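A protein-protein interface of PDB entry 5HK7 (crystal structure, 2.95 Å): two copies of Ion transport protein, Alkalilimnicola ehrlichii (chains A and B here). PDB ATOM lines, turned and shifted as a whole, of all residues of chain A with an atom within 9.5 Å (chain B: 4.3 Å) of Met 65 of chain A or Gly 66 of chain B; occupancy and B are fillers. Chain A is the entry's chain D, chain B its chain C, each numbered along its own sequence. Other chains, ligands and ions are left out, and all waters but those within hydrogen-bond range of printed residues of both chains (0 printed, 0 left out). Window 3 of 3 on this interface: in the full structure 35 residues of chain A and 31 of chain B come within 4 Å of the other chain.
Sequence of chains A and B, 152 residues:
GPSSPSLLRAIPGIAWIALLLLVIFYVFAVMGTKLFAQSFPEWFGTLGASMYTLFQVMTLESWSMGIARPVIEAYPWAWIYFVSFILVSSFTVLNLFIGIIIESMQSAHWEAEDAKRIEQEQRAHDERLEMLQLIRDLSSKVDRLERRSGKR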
ATOM      1  N   TRP A  43      19.405  16.441  10.694  1.00  0.00           N
ATOM      2  CA  TRP A  43      20.097  15.342  10.104  1.00  0.00           C
ATOM      3  C   TRP A  43      19.645  15.084   8.701  1.00  0.00           C
ATOM      4  O   TRP A  43      20.511  14.922   7.881  1.00  0.00           O
ATOM      5  CB  TRP A  43      19.959  14.130  10.972  1.00  0.00           C
ATOM      6  CG  TRP A  43      20.553  14.374  12.317  1.00  0.00           C
ATOM      7  CD1 TRP A  43      21.579  15.271  12.656  1.00  0.00           C
ATOM      8  CD2 TRP A  43      20.210  13.703  13.510  1.00  0.00           C
ATOM      9  NE1 TRP A  43      21.858  15.190  13.997  1.00  0.00           N
ATOM     10  CE2 TRP A  43      21.033  14.228  14.543  1.00  0.00           C
ATOM     11  CE3 TRP A  43      19.288  12.702  13.822  1.00  0.00           C
ATOM     12  CZ2 TRP A  43      20.936  13.777  15.867  1.00  0.00           C
ATOM     13  CZ3 TRP A  43      19.198  12.275  15.129  1.00  0.00           C
ATOM     14  CH2 TRP A  43      20.020  12.806  16.135  1.00  0.00           C
ATOM     15  N   GLN A  56      28.684  10.770   7.470  1.00  0.00           N
ATOM     16  CA  GLN A  56      29.143  10.692   8.823  1.00  0.00           C
ATOM     17  C   GLN A  56      28.882   9.301   9.316  1.00  0.00           C
ATOM     18  O   GLN A  56      29.680   8.779  10.132  1.00  0.00           O
ATOM     19  CB  GLN A  56      28.350  11.637   9.689  1.00  0.00           C
ATOM     20  CG  GLN A  56      28.772  11.615  11.143  1.00  0.00           C
ATOM     21  CD  GLN A  56      27.769  12.295  12.023  1.00  0.00           C
ATOM     22  OE1 GLN A  56      27.154  13.272  11.625  1.00  0.00           O
ATOM     23  NE2 GLN A  56      27.593  11.789  13.221  1.00  0.00           N
ATOM     24  N   VAL A  57      27.747   8.736   8.860  1.00  0.00           N
ATOM     25  CA  VAL A  57      27.372   7.353   9.149  1.00  0.00           C
ATOM     26  C   VAL A  57      28.303   6.407   8.450  1.00  0.00           C
ATOM     27  O   VAL A  57      28.581   5.329   8.963  1.00  0.00           O
ATOM     28  CB  VAL A  57      25.956   6.986   8.693  1.00  0.00           C
ATOM     29  CG1 VAL A  57      25.710   5.514   8.915  1.00  0.00           C
ATOM     30  CG2 VAL A  57      24.899   7.749   9.466  1.00  0.00           C
ATOM     31  N   LEU A  60      31.314   5.878  10.091  1.00  0.00           N
ATOM     32  CA  LEU A  60      30.963   5.068  11.238  1.00  0.00           C
ATOM     33  C   LEU A  60      30.977   5.867  12.528  1.00  0.00           C
ATOM     34  O   LEU A  60      31.181   5.310  13.611  1.00  0.00           O
ATOM     35  CB  LEU A  60      31.952   3.946  11.392  1.00  0.00           C
ATOM     36  CG  LEU A  60      31.620   2.771  10.541  1.00  0.00           C
ATOM     37  CD1 LEU A  60      32.703   1.780  10.874  1.00  0.00           C
ATOM     38  CD2 LEU A  60      30.308   2.171  10.973  1.00  0.00           C
ATOM     39  N   GLU A  61      30.804   7.177  12.405  1.00  0.00           N
ATOM     40  CA  GLU A  61      31.157   8.063  13.475  1.00  0.00           C
ATOM     41  C   GLU A  61      29.910   8.433  14.222  1.00  0.00           C
ATOM     42  O   GLU A  61      29.077   9.120  13.685  1.00  0.00           O
ATOM     43  CB  GLU A  61      31.767   9.300  12.878  1.00  0.00           C
ATOM     44  CG  GLU A  61      32.509  10.154  13.885  1.00  0.00           C
ATOM     45  CD  GLU A  61      31.582  11.105  14.608  1.00  0.00           C
ATOM     46  OE1 GLU A  61      30.873  11.907  13.977  1.00  0.00           O
ATOM     47  OE2 GLU A  61      31.543  11.029  15.829  1.00  0.00           O
ATOM     48  N   SER A  62      29.760   7.996  15.464  1.00  0.00           N
ATOM     49  CA  SER A  62      28.528   8.308  16.158  1.00  0.00           C
ATOM     50  C   SER A  62      27.289   7.844  15.396  1.00  0.00           C
ATOM     51  O   SER A  62      26.259   8.495  15.442  1.00  0.00           O
ATOM     52  CB  SER A  62      28.432   9.807  16.293  1.00  0.00           C
ATOM     53  OG  SER A  62      29.068  10.166  17.464  1.00  0.00           O
ATOM     54  N   TRP A  63      27.390   6.743  14.665  1.00  0.00           N
ATOM     55  CA  TRP A  63      26.312   6.391  13.763  1.00  0.00           C
ATOM     56  C   TRP A  63      25.092   5.946  14.555  1.00  0.00           C
ATOM     57  O   TRP A  63      23.981   6.140  14.113  1.00  0.00           O
ATOM     58  CB  TRP A  63      26.742   5.360  12.721  1.00  0.00           C
ATOM     59  CG  TRP A  63      26.817   3.975  13.211  1.00  0.00           C
ATOM     60  CD1 TRP A  63      27.942   3.316  13.582  1.00  0.00           C
ATOM     61  CD2 TRP A  63      25.735   3.041  13.349  1.00  0.00           C
ATOM     62  NE1 TRP A  63      27.643   2.019  13.954  1.00  0.00           N
ATOM     63  CE2 TRP A  63      26.292   1.828  13.829  1.00  0.00           C
ATOM     64  CE3 TRP A  63      24.351   3.114  13.129  1.00  0.00           C
ATOM     65  CZ2 TRP A  63      25.510   0.703  14.115  1.00  0.00           C
ATOM     66  CZ3 TRP A  63      23.570   2.019  13.432  1.00  0.00           C
ATOM     67  CH2 TRP A  63      24.146   0.821  13.913  1.00  0.00           C
ATOM     68  N   SER A  64      25.310   5.412  15.748  1.00  0.00           N
ATOM     69  CA  SER A  64      24.264   4.798  16.520  1.00  0.00           C
ATOM     70  C   SER A  64      23.860   5.648  17.722  1.00  0.00           C
ATOM     71  O   SER A  64      22.671   6.000  17.909  1.00  0.00           O
ATOM     72  CB  SER A  64      24.764   3.493  17.067  1.00  0.00           C
ATOM     73  OG  SER A  64      23.702   2.584  17.170  1.00  0.00           O
ATOM     74  N   MET A  65      24.837   5.924  18.587  1.00  0.00           N
ATOM     75  CA  MET A  65      24.528   6.624  19.826  1.00  0.00           C
ATOM     76  C   MET A  65      24.134   7.993  19.402  1.00  0.00           C
ATOM     77  O   MET A  65      23.313   8.570  20.067  1.00  0.00           O
ATOM     78  CB  MET A  65      25.709   6.720  20.780  1.00  0.00           C
ATOM     79  CG  MET A  65      26.156   5.355  21.240  1.00  0.00           C
ATOM     80  SD  MET A  65      24.999   4.576  22.371  1.00  0.00           S
ATOM     81  CE  MET A  65      25.388   5.577  23.834  1.00  0.00           C
ATOM     82  N   GLY A  66      24.701   8.478  18.282  1.00  0.00           N
ATOM     83  CA  GLY A  66      24.485   9.834  17.798  1.00  0.00           C
ATOM     84  C   GLY A  66      23.228  10.040  16.962  1.00  0.00           C
ATOM     85  O   GLY A  66      22.404  10.908  17.264  1.00  0.00           O
ATOM     86  N   ILE A  67      23.088   9.246  15.902  1.00  0.00           N
ATOM     87  CA  ILE A  67      22.096   9.468  14.862  1.00  0.00           C
ATOM     88  C   ILE A  67      21.066   8.369  14.867  1.00  0.00           C
ATOM     89  O   ILE A  67      19.885   8.628  14.866  1.00  0.00           O
ATOM     90  CB  ILE A  67      22.700   9.425  13.463  1.00  0.00           C
ATOM     91  CG1 ILE A  67      23.921  10.333  13.343  1.00  0.00           C
ATOM     92  CG2 ILE A  67      21.697   9.865  12.451  1.00  0.00           C
ATOM     93  CD1 ILE A  67      23.622  11.785  13.525  1.00  0.00           C
ATOM     94  N   ALA A  68      21.505   7.124  14.806  1.00  0.00           N
ATOM     95  CA  ALA A  68      20.574   6.013  14.521  1.00  0.00           C
ATOM     96  C   ALA A  68      19.655   5.803  15.667  1.00  0.00           C
ATOM     97  O   ALA A  68      18.508   5.745  15.467  1.00  0.00           O
ATOM     98  CB  ALA A  68      21.296   4.722  14.258  1.00  0.00           C
ATOM     99  N   ARG A  69      20.163   5.685  16.876  1.00  0.00           N
ATOM    100  CA  ARG A  69      19.322   5.330  18.008  1.00  0.00           C
ATOM    101  C   ARG A  69      18.114   6.291  18.168  1.00  0.00           C
ATOM    102  O   ARG A  69      16.955   5.837  18.106  1.00  0.00           O
ATOM    103  CB  ARG A  69      20.153   5.272  19.282  1.00  0.00           C
ATOM    104  CG  ARG A  69      21.150   4.121  19.342  1.00  0.00           C
ATOM    105  CD  ARG A  69      20.859   3.258  20.575  1.00  0.00           C
ATOM    106  NE  ARG A  69      21.986   2.390  20.901  1.00  0.00           N
ATOM    107  CZ  ARG A  69      21.907   1.066  21.081  1.00  0.00           C
ATOM    108  NH1 ARG A  69      20.762   0.388  21.032  1.00  0.00           N
ATOM    109  NH2 ARG A  69      22.997   0.380  21.326  1.00  0.00           N
ATOM    110  N   PRO A  70      18.379   7.609  18.353  1.00  0.00           N
ATOM    111  CA  PRO A  70      17.349   8.641  18.368  1.00  0.00           C
ATOM    112  C   PRO A  70      16.348   8.642  17.221  1.00  0.00           C
ATOM    113  O   PRO A  70      15.163   8.975  17.446  1.00  0.00           O
ATOM    114  CB  PRO A  70      18.144   9.940  18.385  1.00  0.00           C
ATOM    115  CG  PRO A  70      19.533   9.523  18.089  1.00  0.00           C
ATOM    116  CD  PRO A  70      19.654   8.203  18.734  1.00  0.00           C
ATOM    117  N   VAL A  71      16.795   8.270  16.028  1.00  0.00           N
ATOM    118  CA  VAL A  71      15.858   8.099  14.917  1.00  0.00           C
ATOM    119  C   VAL A  71      15.004   6.824  15.014  1.00  0.00           C
ATOM    120  O   VAL A  71      13.934   6.771  14.434  1.00  0.00           O
ATOM    121  CB  VAL A  71      16.600   8.123  13.590  1.00  0.00           C
ATOM    122  CG1 VAL A  71      15.671   7.825  12.407  1.00  0.00           C
ATOM    123  CG2 VAL A  71      17.353   9.439  13.485  1.00  0.00           C
ATOM    124  N   ILE A  72      15.478   5.826  15.763  1.00  0.00           N
ATOM    125  CA  ILE A  72      14.862   4.520  15.837  1.00  0.00           C
ATOM    126  C   ILE A  72      13.848   4.594  16.915  1.00  0.00           C
ATOM    127  O   ILE A  72      13.044   3.698  17.103  1.00  0.00           O
ATOM    128  CB  ILE A  72      15.895   3.447  16.205  1.00  0.00           C
ATOM    129  CG1 ILE A  72      16.853   3.226  15.051  1.00  0.00           C
ATOM    130  CG2 ILE A  72      15.252   2.099  16.333  1.00  0.00           C
ATOM    131  CD1 ILE A  72      18.034   2.331  15.365  1.00  0.00           C
ATOM    132  N   PHE A  82      19.783   1.983   8.819  1.00  0.00           N
ATOM    133  CA  PHE A  82      21.168   2.296   9.159  1.00  0.00           C
ATOM    134  C   PHE A  82      22.021   1.056   9.103  1.00  0.00           C
ATOM    135  O   PHE A  82      23.161   1.133   8.705  1.00  0.00           O
ATOM    136  CB  PHE A  82      21.283   2.926  10.526  1.00  0.00           C
ATOM    137  CG  PHE A  82      20.636   4.246  10.616  1.00  0.00           C
ATOM    138  CD1 PHE A  82      21.376   5.406  10.384  1.00  0.00           C
ATOM    139  CD2 PHE A  82      19.300   4.350  10.933  1.00  0.00           C
ATOM    140  CE1 PHE A  82      20.806   6.674  10.491  1.00  0.00           C
ATOM    141  CE2 PHE A  82      18.709   5.600  11.032  1.00  0.00           C
ATOM    142  CZ  PHE A  82      19.463   6.765  10.809  1.00  0.00           C
ATOM    143  N   TRP B  43      19.582  -1.381  25.763  1.00  0.00           N
ATOM    144  CA  TRP B  43      20.677  -1.885  24.998  1.00  0.00           C
ATOM    145  C   TRP B  43      20.593  -3.354  24.803  1.00  0.00           C
ATOM    146  O   TRP B  43      20.893  -3.822  23.733  1.00  0.00           O
ATOM    147  CB  TRP B  43      21.964  -1.600  25.701  1.00  0.00           C
ATOM    148  CG  TRP B  43      22.245  -0.189  25.783  1.00  0.00           C
ATOM    149  CD1 TRP B  43      21.784   0.758  24.976  1.00  0.00           C
ATOM    150  CD2 TRP B  43      23.082   0.453  26.721  1.00  0.00           C
ATOM    151  NE1 TRP B  43      22.272   1.970  25.337  1.00  0.00           N
ATOM    152  CE2 TRP B  43      23.081   1.800  26.419  1.00  0.00           C
ATOM    153  CE3 TRP B  43      23.860   0.007  27.769  1.00  0.00           C
ATOM    154  CZ2 TRP B  43      23.807   2.723  27.136  1.00  0.00           C
ATOM    155  CZ3 TRP B  43      24.578   0.902  28.473  1.00  0.00           C
ATOM    156  CH2 TRP B  43      24.551   2.256  28.162  1.00  0.00           C
ATOM    157  N   GLN B  56      26.454  -2.291  16.719  1.00  0.00           N
ATOM    158  CA  GLN B  56      27.080  -1.080  17.217  1.00  0.00           C
ATOM    159  C   GLN B  56      28.445  -1.294  17.729  1.00  0.00           C
ATOM    160  O   GLN B  56      29.347  -0.563  17.343  1.00  0.00           O
ATOM    161  CB  GLN B  56      26.329  -0.509  18.387  1.00  0.00           C
ATOM    162  CG  GLN B  56      26.277   0.983  18.262  1.00  0.00           C
ATOM    163  CD  GLN B  56      26.069   1.655  19.564  1.00  0.00           C
ATOM    164  OE1 GLN B  56      24.932   1.917  19.952  1.00  0.00           O
ATOM    165  NE2 GLN B  56      27.168   1.959  20.257  1.00  0.00           N
ATOM    166  N   GLU B  61      31.696   1.626  17.499  1.00  0.00           N
ATOM    167  CA  GLU B  61      31.007   2.905  17.513  1.00  0.00           C
ATOM    168  C   GLU B  61      30.636   3.129  18.945  1.00  0.00           C
ATOM    169  O   GLU B  61      29.635   2.564  19.468  1.00  0.00           O
ATOM    170  CB  GLU B  61      29.748   2.925  16.630  1.00  0.00           C
ATOM    171  CG  GLU B  61      29.196   4.320  16.283  1.00  0.00           C
ATOM    172  CD  GLU B  61      28.590   5.109  17.462  1.00  0.00           C
ATOM    173  OE1 GLU B  61      27.330   5.140  17.601  1.00  0.00           O
ATOM    174  OE2 GLU B  61      29.382   5.734  18.231  1.00  0.00           O
ATOM    175  N   SER B  62      31.460   3.952  19.576  1.00  0.00           N
ATOM    176  CA  SER B  62      31.128   4.432  20.863  1.00  0.00           C
ATOM    177  C   SER B  62      31.051   3.245  21.866  1.00  0.00           C
ATOM    178  O   SER B  62      30.245   3.247  22.784  1.00  0.00           O
ATOM    179  CB  SER B  62      29.824   5.172  20.703  1.00  0.00           C
ATOM    180  OG  SER B  62      29.213   5.417  21.924  1.00  0.00           O
ATOM    181  N   SER B  64      32.724   1.908  24.080  1.00  0.00           N
ATOM    182  CA  SER B  64      33.229   1.838  25.405  1.00  0.00           C
ATOM    183  C   SER B  64      32.736   2.962  26.196  1.00  0.00           C
ATOM    184  O   SER B  64      32.394   2.743  27.346  1.00  0.00           O
ATOM    185  CB  SER B  64      34.737   1.826  25.478  1.00  0.00           C
ATOM    186  OG  SER B  64      35.097   1.507  26.811  1.00  0.00           O
ATOM    187  N   MET B  65      32.743   4.172  25.638  1.00  0.00           N
ATOM    188  CA  MET B  65      32.361   5.280  26.483  1.00  0.00           C
ATOM    189  C   MET B  65      30.886   5.091  26.573  1.00  0.00           C
ATOM    190  O   MET B  65      30.316   5.273  27.640  1.00  0.00           O
ATOM    191  CB  MET B  65      32.674   6.660  25.903  1.00  0.00           C
ATOM    192  CG  MET B  65      34.098   7.135  26.066  1.00  0.00           C
ATOM    193  SD  MET B  65      34.692   6.774  27.695  1.00  0.00           S
ATOM    194  CE  MET B  65      36.372   7.289  27.444  1.00  0.00           C
ATOM    195  N   GLY B  66      30.289   4.685  25.453  1.00  0.00           N
ATOM    196  CA  GLY B  66      28.846   4.652  25.313  1.00  0.00           C
ATOM    197  C   GLY B  66      28.176   3.470  25.973  1.00  0.00           C
ATOM    198  O   GLY B  66      27.177   3.645  26.655  1.00  0.00           O
ATOM    199  N   ILE B  67      28.700   2.267  25.755  1.00  0.00           N
ATOM    200  CA  ILE B  67      28.091   1.049  26.281  1.00  0.00           C
ATOM    201  C   ILE B  67      28.993   0.490  27.362  1.00  0.00           C
ATOM    202  O   ILE B  67      28.629   0.522  28.532  1.00  0.00           O
ATOM    203  CB  ILE B  67      27.868  -0.033  25.194  1.00  0.00           C
ATOM    204  CG1 ILE B  67      26.596   0.227  24.433  1.00  0.00           C
ATOM    205  CG2 ILE B  67      27.625  -1.378  25.813  1.00  0.00           C
ATOM    206  CD1 ILE B  67      26.559   1.592  23.807  1.00  0.00           C
ATOM    207  N   ALA B  68      30.155  -0.045  26.981  1.00  0.00           N
ATOM    208  CA  ALA B  68      30.817  -1.000  27.859  1.00  0.00           C
ATOM    209  C   ALA B  68      31.117  -0.394  29.229  1.00  0.00           C
ATOM    210  O   ALA B  68      30.907  -1.062  30.206  1.00  0.00           O
ATOM    211  CB  ALA B  68      32.064  -1.575  27.241  1.00  0.00           C
ATOM    212  N   PRO B  70      29.774   1.969  31.081  1.00  0.00           N
ATOM    213  CA  PRO B  70      28.535   1.902  31.843  1.00  0.00           C
ATOM    214  C   PRO B  70      28.073   0.548  32.287  1.00  0.00           C
ATOM    215  O   PRO B  70      27.510   0.459  33.362  1.00  0.00           O
ATOM    216  CB  PRO B  70      27.518   2.427  30.865  1.00  0.00           C
ATOM    217  CG  PRO B  70      28.261   3.466  30.149  1.00  0.00           C
ATOM    218  CD  PRO B  70      29.719   3.103  30.153  1.00  0.00           C
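OE1 of Gln 56 of chain B lies within hydrogen-bond range of OG of Ser 64 of chain A (3.1 Å).
SD of Met 65 of chain A sits close to OE1 of Gln 56 of chain B (3.6 Å).
The guanidinium group (NH2) of Arg 69 of chain A lies within hydrogen-bond range of the side-chain amide oxygen (OE1) of Gln 56 of chain B, at 2.8 Å.
The backbone NH (N) of Trp 63 of chain A sits at hydrogen-bond distance from the side-chain carboxylate (OE1) of Glu 61 of chain B, at 3.3 Å.
The backbone NH (N) of Ser 64 of chain A sits at hydrogen-bond distance from the side-chain carboxylate (OE1) of Glu 61 of chain B (2.8 Å).
OE1 of Glu 61 of chain B sits at hydrogen-bond distance from N of Met 65 of chain A, 2.8 Å away.
The side-chain amide nitrogen (NE2) of Gln 56 of chain B lies within hydrogen-bond range of the backbone carbonyl oxygen (O) of Glu 61 of chain B, 2.7 Å away.
The backbone carbonyl oxygen (O) of Ser 62 of chain B lies within hydrogen-bond range of the backbone NH (N) of Ile 67 of chain B (3.5 Å).
OG of Ser 62 of chain A is in hydrogen-bond range of OE2 of Glu 61 of chain A (3.1 Å).
The backbone carbonyl oxygen of Ser 62 of chain A sits at hydrogen-bond distance from the backbone NH of Ile 67 of chain A, at 3.3 Å.
O of Trp 63 of chain A lies within hydrogen-bond range of N of Ala 68 of chain A.
O of Ser 64 of chain A lies within hydrogen-bond range of N of Arg 69 of chain A (2.7 Å).
Among the printed residues, pairs that only touch across the chains: Leu 60 of chain A with Glu 61 of chain B, Ser 62 of chain A with Glu 61 of chain B, Trp 63 of chain A with Gln 56 of chain B, Met 65 of chain A with Ser 62 of chain B, Met 65 of chain A with Gly 66 of chain B, Met 65 of chain A with Ile 67 of chain B and Arg 69 of chain A with Trp 43 of chain B.
Of the printed residues of chain B, Leu 60 of chain A touches Glu 61.
Of the printed residues of chain B, Ser 62 of chain A touches Glu 61 (3.4 Å).
Of chain B, only Gln 56 (3.6 Å), Glu 61 (2.8 Å), Ser 62 (3.1 Å), Gly 66 (3.9 Å) and Ile 67 (3.7 Å) come within 4 Å of Met 65 of chain A.
Gly 66 of chain A touches none of the printed residues of chain B.
Ile 67 of chain A touches none of the printed residues of chain B.
Of the printed residues of chain A, Glu 61 of chain B touches Leu 60 (3.5 Å), Ser 62 (3.4 Å), Trp 63 (3.1 Å), Ser 64 (2.8 Å) and Met 65 (2.8 Å).
Gly 66 of chain B touches just one residue of chain A: Met 65 (3.9 Å).
Of the printed residues of chain A, Ile 67 of chain B touches Met 65.
The nearest printed residue of chain B that does not touch Met 65 of chain A is Trp 43 of chain B (4.6 Å).
The nearest residue of chain A that does not touch Gly 66 of chain B is Arg 69 of chain A (7.5 Å).
Of the 17 printed residues of chain A, 6 touch a printed residue of chain B.
Hydrophobic or aromatic side chains of chain A within 4 Å of the printed part of chain B: Trp 63 and Met 65.
Of the 10 printed residues of chain B, 6 touch a printed residue of chain A.
Among the printed residues, 13 pairs touch across the chains.
Ser 64 of chain A touches Gln 56 of chain B, but with the chains exchanged Gln 56 of chain A does not touch Ser 64 of chain B (15.6 Å).
Met 65 of chain A touches Gln 56 of chain B, but with the chains exchanged Gln 56 of chain A does not touch Met 65 of chain B (14.6 Å).
Met 65 of chain A touches Glu 61 of chain B, but with the chains exchanged Glu 61 of chain A does not touch Met 65 of chain B (11.0 Å).
Met 65 of chain A touches Ile 67 of chain B, but with the chains exchanged Ile 67 of chain A does not touch Met 65 of chain B (13.9 Å).
Positions printed for both chains: 43, 56, 61, 62, 64, 65, 66, 67, 68 and 70.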
